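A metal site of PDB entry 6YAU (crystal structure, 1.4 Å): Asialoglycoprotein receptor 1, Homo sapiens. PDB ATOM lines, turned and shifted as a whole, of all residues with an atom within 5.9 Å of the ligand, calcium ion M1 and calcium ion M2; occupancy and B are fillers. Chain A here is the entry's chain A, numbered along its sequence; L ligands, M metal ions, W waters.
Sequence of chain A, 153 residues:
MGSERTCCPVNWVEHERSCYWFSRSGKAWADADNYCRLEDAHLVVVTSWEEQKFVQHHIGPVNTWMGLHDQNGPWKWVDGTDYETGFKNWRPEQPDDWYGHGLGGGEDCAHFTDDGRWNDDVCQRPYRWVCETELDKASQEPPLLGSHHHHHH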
ATOM      1  N   ASN A  63     -12.824  22.838   1.021  1.00  0.00           N
ATOM      2  CA  ASN A  63     -12.521  22.913  -0.418  1.00  0.00           C
ATOM      3  C   ASN A  63     -11.456  21.878  -0.726  1.00  0.00           C
ATOM      4  O   ASN A  63     -10.407  21.902  -0.095  1.00  0.00           O
ATOM      5  CB  ASN A  63     -12.037  24.297  -0.813  1.00  0.00           C
ATOM      6  CG  ASN A  63     -13.154  25.290  -0.842  1.00  0.00           C
ATOM      7  OD1 ASN A  63     -13.007  26.455  -0.443  1.00  0.00           O
ATOM      8  ND2 ASN A  63     -14.279  24.854  -1.365  1.00  0.00           N
ATOM      9  N   ASP A  70     -10.168  21.472 -17.053  1.00  0.00           N
ATOM     10  CA  ASP A  70     -10.311  21.904 -18.448  1.00  0.00           C
ATOM     11  C   ASP A  70      -9.165  22.837 -18.875  1.00  0.00           C
ATOM     12  O   ASP A  70      -9.388  23.754 -19.644  1.00  0.00           O
ATOM     13  CB  ASP A  70     -11.707  22.501 -18.748  1.00  0.00           C
ATOM     14  CG  ASP A  70     -11.935  23.921 -18.267  1.00  0.00           C
ATOM     15  OD1 ASP A  70     -11.218  24.366 -17.366  1.00  0.00           O
ATOM     16  OD2 ASP A  70     -12.859  24.591 -18.787  1.00  0.00           O
ATOM     17  N   TRP A  75     -13.582  19.824 -20.541  1.00  0.00           N
ATOM     18  CA  TRP A  75     -13.501  19.180 -19.230  1.00  0.00           C
ATOM     19  C   TRP A  75     -13.167  17.718 -19.388  1.00  0.00           C
ATOM     20  O   TRP A  75     -13.784  17.034 -20.215  1.00  0.00           O
ATOM     21  CB  TRP A  75     -14.815  19.344 -18.453  1.00  0.00           C
ATOM     22  CG  TRP A  75     -14.978  20.718 -17.870  1.00  0.00           C
ATOM     23  CD1 TRP A  75     -15.694  21.761 -18.390  1.00  0.00           C
ATOM     24  CD2 TRP A  75     -14.364  21.204 -16.683  1.00  0.00           C
ATOM     25  NE1 TRP A  75     -15.545  22.877 -17.605  1.00  0.00           N
ATOM     26  CE2 TRP A  75     -14.705  22.563 -16.546  1.00  0.00           C
ATOM     27  CE3 TRP A  75     -13.497  20.627 -15.727  1.00  0.00           C
ATOM     28  CZ2 TRP A  75     -14.290  23.338 -15.457  1.00  0.00           C
ATOM     29  CZ3 TRP A  75     -13.068  21.403 -14.657  1.00  0.00           C
ATOM     30  CH2 TRP A  75     -13.420  22.750 -14.558  1.00  0.00           C
ATOM     31  N   ARG A  91     -22.281  22.873  -8.522  1.00  0.00           N
ATOM     32  CA  ARG A  91     -23.194  23.775  -7.839  1.00  0.00           C
ATOM     33  C   ARG A  91     -23.929  24.505  -8.975  1.00  0.00           C
ATOM     34  O   ARG A  91     -23.283  24.846  -9.975  1.00  0.00           O
ATOM     35  CB  ARG A  91     -22.441  24.805  -6.988  1.00  0.00           C
ATOM     36  CG  ARG A  91     -23.389  25.771  -6.239  1.00  0.00           C
ATOM     37  CD  ARG A  91     -22.691  26.606  -5.209  1.00  0.00           C
ATOM     38  NE  ARG A  91     -21.796  27.581  -5.818  1.00  0.00           N
ATOM     39  CZ  ARG A  91     -20.540  27.791  -5.440  1.00  0.00           C
ATOM     40  NH1 ARG A  91     -20.010  27.083  -4.448  1.00  0.00           N
ATOM     41  NH2 ARG A  91     -19.812  28.725  -6.036  1.00  0.00           N
ATOM     42  N   GLN A  94     -22.427  26.627 -12.023  1.00  0.00           N
ATOM     43  CA  GLN A  94     -21.035  26.250 -12.213  1.00  0.00           C
ATOM     44  C   GLN A  94     -21.039  25.109 -13.241  1.00  0.00           C
ATOM     45  O   GLN A  94     -22.053  24.399 -13.349  1.00  0.00           O
ATOM     46  CB  GLN A  94     -20.365  25.821 -10.890  1.00  0.00           C
ATOM     47  CG  GLN A  94     -20.429  26.878  -9.781  1.00  0.00           C
ATOM     48  CD  GLN A  94     -19.616  28.149 -10.015  1.00  0.00           C
ATOM     49  OE1 GLN A  94     -18.683  28.207 -10.841  1.00  0.00           O
ATOM     50  NE2 GLN A  94     -19.958  29.200  -9.273  1.00  0.00           N
ATOM     51  N   PRO A  95     -19.953  24.899 -14.006  1.00  0.00           N
ATOM     52  CA  PRO A  95     -18.705  25.688 -14.027  1.00  0.00           C
ATOM     53  C   PRO A  95     -18.896  27.032 -14.739  1.00  0.00           C
ATOM     54  O   PRO A  95     -19.632  27.084 -15.697  1.00  0.00           O
ATOM     55  CB  PRO A  95     -17.738  24.778 -14.787  1.00  0.00           C
ATOM     56  CG  PRO A  95     -18.593  23.947 -15.703  1.00  0.00           C
ATOM     57  CD  PRO A  95     -19.961  23.850 -15.051  1.00  0.00           C
ATOM     58  N   ASP A  96     -18.268  28.114 -14.261  1.00  0.00           N
ATOM     59  CA  ASP A  96     -18.457  29.416 -14.907  1.00  0.00           C
ATOM     60  C   ASP A  96     -17.173  29.989 -15.539  1.00  0.00           C
ATOM     61  O   ASP A  96     -17.239  31.041 -16.156  1.00  0.00           O
ATOM     62  CB  ASP A  96     -19.084  30.426 -13.930  1.00  0.00           C
ATOM     63  CG  ASP A  96     -18.254  30.690 -12.693  1.00  0.00           C
ATOM     64  OD1 ASP A  96     -17.212  30.054 -12.543  1.00  0.00           O
ATOM     65  OD2 ASP A  96     -18.647  31.540 -11.878  1.00  0.00           O
ATOM     66  N   ASP A  97     -16.024  29.316 -15.384  1.00  0.00           N
ATOM     67  CA  ASP A  97     -14.738  29.807 -15.942  1.00  0.00           C
ATOM     68  C   ASP A  97     -14.523  31.280 -15.576  1.00  0.00           C
ATOM     69  O   ASP A  97     -14.126  32.074 -16.433  1.00  0.00           O
ATOM     70  CB  ASP A  97     -14.703  29.651 -17.482  1.00  0.00           C
ATOM     71  CG  ASP A  97     -13.306  29.678 -18.065  1.00  0.00           C
ATOM     72  OD1 ASP A  97     -12.398  29.020 -17.491  1.00  0.00           O
ATOM     73  OD2 ASP A  97     -13.123  30.360 -19.114  1.00  0.00           O
ATOM     74  N   TRP A  98     -14.791  31.634 -14.318  1.00  0.00           N
ATOM     75  CA  TRP A  98     -14.732  33.025 -13.834  1.00  0.00           C
ATOM     76  C   TRP A  98     -13.385  33.723 -14.011  1.00  0.00           C
ATOM     77  O   TRP A  98     -12.330  33.144 -13.692  1.00  0.00           O
ATOM     78  CB  TRP A  98     -15.174  33.080 -12.376  1.00  0.00           C
ATOM     79  CG  TRP A  98     -15.462  34.433 -11.787  1.00  0.00           C
ATOM     80  CD1 TRP A  98     -16.289  35.399 -12.297  1.00  0.00           C
ATOM     81  CD2 TRP A  98     -15.087  34.892 -10.479  1.00  0.00           C
ATOM     82  NE1 TRP A  98     -16.397  36.450 -11.419  1.00  0.00           N
ATOM     83  CE2 TRP A  98     -15.698  36.149 -10.269  1.00  0.00           C
ATOM     84  CE3 TRP A  98     -14.232  34.377  -9.481  1.00  0.00           C
ATOM     85  CZ2 TRP A  98     -15.472  36.908  -9.114  1.00  0.00           C
ATOM     86  CZ3 TRP A  98     -14.056  35.104  -8.301  1.00  0.00           C
ATOM     87  CH2 TRP A  98     -14.690  36.344  -8.122  1.00  0.00           C
ATOM     88  N   GLY A 106      -9.135  32.120 -16.524  1.00  0.00           N
ATOM     89  CA  GLY A 106     -10.454  31.752 -16.044  1.00  0.00           C
ATOM     90  C   GLY A 106     -10.298  30.868 -14.833  1.00  0.00           C
ATOM     91  O   GLY A 106      -9.548  31.202 -13.916  1.00  0.00           O
ATOM     92  N   GLU A 107     -10.990  29.717 -14.847  1.00  0.00           N
ATOM     93  CA  GLU A 107     -10.942  28.742 -13.753  1.00  0.00           C
ATOM     94  C   GLU A 107     -10.927  27.381 -14.405  1.00  0.00           C
ATOM     95  O   GLU A 107     -11.827  27.027 -15.148  1.00  0.00           O
ATOM     96  CB  GLU A 107     -12.153  28.921 -12.827  1.00  0.00           C
ATOM     97  CG  GLU A 107     -12.106  30.188 -11.968  1.00  0.00           C
ATOM     98  CD  GLU A 107     -13.319  30.377 -11.078  1.00  0.00           C
ATOM     99  OE1 GLU A 107     -13.170  30.866  -9.939  1.00  0.00           O
ATOM    100  OE2 GLU A 107     -14.427  29.998 -11.518  1.00  0.00           O
ATOM    101  N   ASP A 108      -9.886  26.612 -14.168  1.00  0.00           N
ATOM    102  CA  ASP A 108      -9.746  25.380 -14.920  1.00  0.00           C
ATOM    103  C   ASP A 108      -9.665  24.117 -14.090  1.00  0.00           C
ATOM    104  O   ASP A 108      -9.505  23.048 -14.677  1.00  0.00           O
ATOM    105  CB  ASP A 108      -8.502  25.482 -15.830  1.00  0.00           C
ATOM    106  CG  ASP A 108      -8.587  26.548 -16.909  1.00  0.00           C
ATOM    107  OD1 ASP A 108      -9.727  27.008 -17.224  1.00  0.00           O
ATOM    108  OD2 ASP A 108      -7.530  26.935 -17.429  1.00  0.00           O
ATOM    109  N   HIS A 111     -13.149  21.395  -7.800  1.00  0.00           N
ATOM    110  CA  HIS A 111     -13.009  21.008  -6.401  1.00  0.00           C
ATOM    111  C   HIS A 111     -14.368  20.783  -5.763  1.00  0.00           C
ATOM    112  O   HIS A 111     -15.392  21.295  -6.250  1.00  0.00           O
ATOM    113  CB  HIS A 111     -12.206  22.050  -5.605  1.00  0.00           C
ATOM    114  CG  HIS A 111     -12.883  23.374  -5.465  1.00  0.00           C
ATOM    115  ND1 HIS A 111     -13.474  23.798  -4.270  1.00  0.00           N
ATOM    116  CD2 HIS A 111     -12.995  24.376  -6.375  1.00  0.00           C
ATOM    117  CE1 HIS A 111     -13.944  25.010  -4.509  1.00  0.00           C
ATOM    118  NE2 HIS A 111     -13.698  25.398  -5.757  1.00  0.00           N
ATOM    119  N   THR A 113     -16.808  21.748  -2.899  1.00  0.00           N
ATOM    120  CA  THR A 113     -16.947  22.936  -2.056  1.00  0.00           C
ATOM    121  C   THR A 113     -17.338  22.399  -0.658  1.00  0.00           C
ATOM    122  O   THR A 113     -17.516  21.174  -0.485  1.00  0.00           O
ATOM    123  CB  THR A 113     -18.036  23.867  -2.606  1.00  0.00           C
ATOM    124  OG1 THR A 113     -19.289  23.167  -2.552  1.00  0.00           O
ATOM    125  CG2 THR A 113     -17.728  24.366  -4.018  1.00  0.00           C
ATOM    126  N   ASN A 119     -17.240  23.100  -7.917  1.00  0.00           N
ATOM    127  CA  ASN A 119     -16.962  24.428  -8.463  1.00  0.00           C
ATOM    128  C   ASN A 119     -15.655  24.364  -9.245  1.00  0.00           C
ATOM    129  O   ASN A 119     -14.756  23.568  -8.908  1.00  0.00           O
ATOM    130  CB  ASN A 119     -16.830  25.460  -7.346  1.00  0.00           C
ATOM    131  CG  ASN A 119     -16.392  26.838  -7.854  1.00  0.00           C
ATOM    132  OD1 ASN A 119     -17.020  27.423  -8.740  1.00  0.00           O
ATOM    133  ND2 ASN A 119     -15.297  27.355  -7.341  1.00  0.00           N
ATOM    134  N   ASP A 120     -15.598  25.114 -10.342  1.00  0.00           N
ATOM    135  CA  ASP A 120     -14.340  25.262 -11.022  1.00  0.00           C
ATOM    136  C   ASP A 120     -13.637  26.471 -10.380  1.00  0.00           C
ATOM    137  O   ASP A 120     -14.250  27.518 -10.113  1.00  0.00           O
ATOM    138  CB  ASP A 120     -14.508  25.457 -12.553  1.00  0.00           C
ATOM    139  CG  ASP A 120     -15.357  26.631 -13.046  1.00  0.00           C
ATOM    140  OD1 ASP A 120     -16.197  27.167 -12.234  1.00  0.00           O
ATOM    141  OD2 ASP A 120     -15.214  26.998 -14.241  1.00  0.00           O
ATOM    142  N   ASP A 121     -12.310  26.328 -10.205  1.00  0.00           N
ATOM    143  CA  ASP A 121     -11.562  27.402  -9.572  1.00  0.00           C
ATOM    144  C   ASP A 121     -10.166  27.538 -10.154  1.00  0.00           C
ATOM    145  O   ASP A 121      -9.740  26.746 -11.000  1.00  0.00           O
ATOM    146  CB  ASP A 121     -11.543  27.166  -8.017  1.00  0.00           C
ATOM    147  CG  ASP A 121     -11.497  28.431  -7.133  1.00  0.00           C
ATOM    148  OD1 ASP A 121     -12.013  28.376  -5.974  1.00  0.00           O
ATOM    149  OD2 ASP A 121     -10.965  29.451  -7.598  1.00  0.00           O
ATOM    150  N   TYR A 127      -5.527  23.949  -2.059  1.00  0.00           N
ATOM    151  CA  TYR A 127      -6.648  23.234  -1.433  1.00  0.00           C
ATOM    152  C   TYR A 127      -6.192  21.814  -0.989  1.00  0.00           C
ATOM    153  O   TYR A 127      -5.181  21.277  -1.500  1.00  0.00           O
ATOM    154  CB  TYR A 127      -7.812  23.045  -2.421  1.00  0.00           C
ATOM    155  CG  TYR A 127      -8.639  24.282  -2.752  1.00  0.00           C
ATOM    156  CD1 TYR A 127      -8.854  25.277  -1.801  1.00  0.00           C
ATOM    157  CD2 TYR A 127      -9.311  24.389  -3.971  1.00  0.00           C
ATOM    158  CE1 TYR A 127      -9.654  26.383  -2.085  1.00  0.00           C
ATOM    159  CE2 TYR A 127     -10.118  25.484  -4.260  1.00  0.00           C
ATOM    160  CZ  TYR A 127     -10.297  26.480  -3.307  1.00  0.00           C
ATOM    161  OH  TYR A 127     -11.122  27.540  -3.554  1.00  0.00           O
HETATM  162  C1  LIG L   1     -15.956  31.881  -1.558  1.00  0.00           C
HETATM  163  C2  LIG L   1     -17.311  32.495  -1.838  1.00  0.00           C
HETATM  164  C3  LIG L   1     -18.372  31.488  -2.292  1.00  0.00           C
HETATM  165  C4  LIG L   1     -19.455  32.092  -3.175  1.00  0.00           C
HETATM  166  C5  LIG L   1     -18.959  32.574  -4.529  1.00  0.00           C
HETATM  167  C6  LIG L   1     -17.468  32.927  -8.411  1.00  0.00           C
HETATM  168  C7  LIG L   1     -16.650  31.797  -9.038  1.00  0.00           C
HETATM  169  C8  LIG L   1     -15.786  31.117  -7.975  1.00  0.00           C
HETATM  170  C9  LIG L   1     -16.617  30.728  -6.751  1.00  0.00           C
HETATM  171  N1  LIG L   1     -14.919  32.482  -2.134  1.00  0.00           N
HETATM  172  O1  LIG L   1     -15.844  30.883  -0.849  1.00  0.00           O
HETATM  173  O2  LIG L   1     -18.313  31.491  -5.207  1.00  0.00           O
HETATM  174  C10 LIG L   1     -17.496  31.886  -6.271  1.00  0.00           C
HETATM  175  O3  LIG L   1     -18.278  32.393  -7.333  1.00  0.00           O
HETATM  176  C11 LIG L   1     -18.394  33.605  -9.402  1.00  0.00           C
HETATM  177  O4  LIG L   1     -19.029  34.747  -8.825  1.00  0.00           O
HETATM  178  O5  LIG L   1     -17.521  30.843  -9.636  1.00  0.00           O
HETATM  179  O6  LIG L   1     -15.204  29.947  -8.515  1.00  0.00           O
HETATM  180  N2  LIG L   1     -15.766  30.238  -5.686  1.00  0.00           N
HETATM  181  C12 LIG L   1     -16.080  29.219  -4.878  1.00  0.00           C
HETATM  182  C13 LIG L   1     -15.035  28.818  -3.885  1.00  0.00           C
HETATM  183  O7  LIG L   1     -17.159  28.619  -4.971  1.00  0.00           O
HETATM  184 CA    CA M   1     -16.326  28.840 -10.605  1.00  0.00          CA
HETATM  185 CA    CA M   2     -12.164  26.585 -17.634  1.00  0.00          CA
HETATM  186  O   HOH W   1     -12.901  30.980  -5.486  1.00  0.00           O
HETATM  187  O   HOH W   2     -13.509  29.346  -0.345  1.00  0.00           O
HETATM  188  O   HOH W   3     -11.963  32.138  -3.230  1.00  0.00           O
HETATM  189  O   HOH W   4     -10.790  26.798 -19.760  1.00  0.00           O
HETATM  190  O   HOH W   5     -13.399  27.221 -19.753  1.00  0.00           O
HETATM  191  O   HOH W   6     -17.931  27.556  -2.382  1.00  0.00           O
HETATM  192  O   HOH W   7     -14.278  26.525 -16.732  1.00  0.00           O
HETATM  193  O   HOH W   8     -15.078  34.472  -4.317  1.00  0.00           O
HETATM  194  O   HOH W   9     -20.759  31.231  -7.210  1.00  0.00           O
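Calcium ion M1 is bound by the side-chain carboxylate of Asp 120 (2.3 Å), the side-chain carboxylate of Glu 107 (2.4 Å), the side-chain amide oxygen of Asn 119 (2.4 Å), the side-chain carboxylate of Asp 96 (2.5 Å), the side-chain amide oxygen of Gln 94 (2.5 Å), the backbone carbonyl oxygen of Asp 120 (2.5 Å), an oxygen (O5) of the ligand (2.5 Å) and an oxygen (O6) of the ligand (2.6 Å).
The side-chain carboxylate of Glu 107 sits close to the backbone NH of Trp 98 (3.3 Å). The backbone NH (N) of Asp 108 is in hydrogen-bond range of the backbone carbonyl oxygen (O) of Asp 121, at 3.2 Å. OH of Tyr 127 is in hydrogen-bond range of OD1 of Asp 121 (2.7 Å). The side-chain amide nitrogen (NE2) of Gln 94 sits close to the guanidinium group (NH2) of Arg 91 (3.3 Å). The side-chain carboxylate of Asp 96 sits close to the backbone NH of Trp 98, at 3.4 Å. The indole nitrogen of Trp 75 sits close to the side-chain carboxylate of Asp 70, at 3.4 Å. The backbone carbonyl oxygen (O) of Asn 119 lies within hydrogen-bond range of the backbone NH (N) of His 111. N of Asp 97 is in hydrogen-bond range of OD2 of Asp 120 (2.7 Å).
Of the 18 residues printed, 4 come within 4 Å of calcium ion M2. Along chain A the residues within 4 Å of calcium ion M2 span positions 70 to 108.
Water W9 lies within hydrogen-bond range of an oxygen (O3) of the ligand, the guanidinium group (NH2) of Arg 91 and the side-chain amide nitrogen (NE2) of Gln 94. Water W2 bridges an oxygen (O1) of the ligand (2.8 Å) and the side-chain amide oxygen of Asn 63 (2.9 Å). Water W6 bridges O7 of the ligand (2.9 Å) and NH1 of Arg 91 (3.0 Å). Water W1 lies within hydrogen-bond range of the side-chain carboxylate of Asp 121 and a nitrogen (N2) of the ligand.
Trp 98 touches the ligand. OD1 of Asp 121 touches C13 of the ligand (3.7 Å). Hydrophobic or aromatic side chains within 4 Å of the ligand: Trp 98. Of the 18 residues printed, 8 come within 4 Å of the ligand.
The guanidinium group of Arg 91 sits at hydrogen-bond distance from an oxygen (O7) of the ligand (2.9 Å).
Calcium ion M2 is bound by water W7 (2.3 Å), the side-chain carboxylate (OD2) of Asp 70 (2.4 Å), the side-chain carboxylate (OD1) of Asp 70 (2.4 Å), the side-chain carboxylate (OD1) of Asp 97 (2.5 Å), the side-chain carboxylate (OD1) of Asp 108 (2.5 Å), water W5 (2.5 Å), water W4 (2.5 Å) and the backbone carbonyl oxygen (O) of Glu 107 (2.5 Å).
Of the 18 residues printed, 5 come within 4 Å of calcium ion M1. The nearest printed residue that does not touch calcium ion M1 is Trp 98 (4.7 Å).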
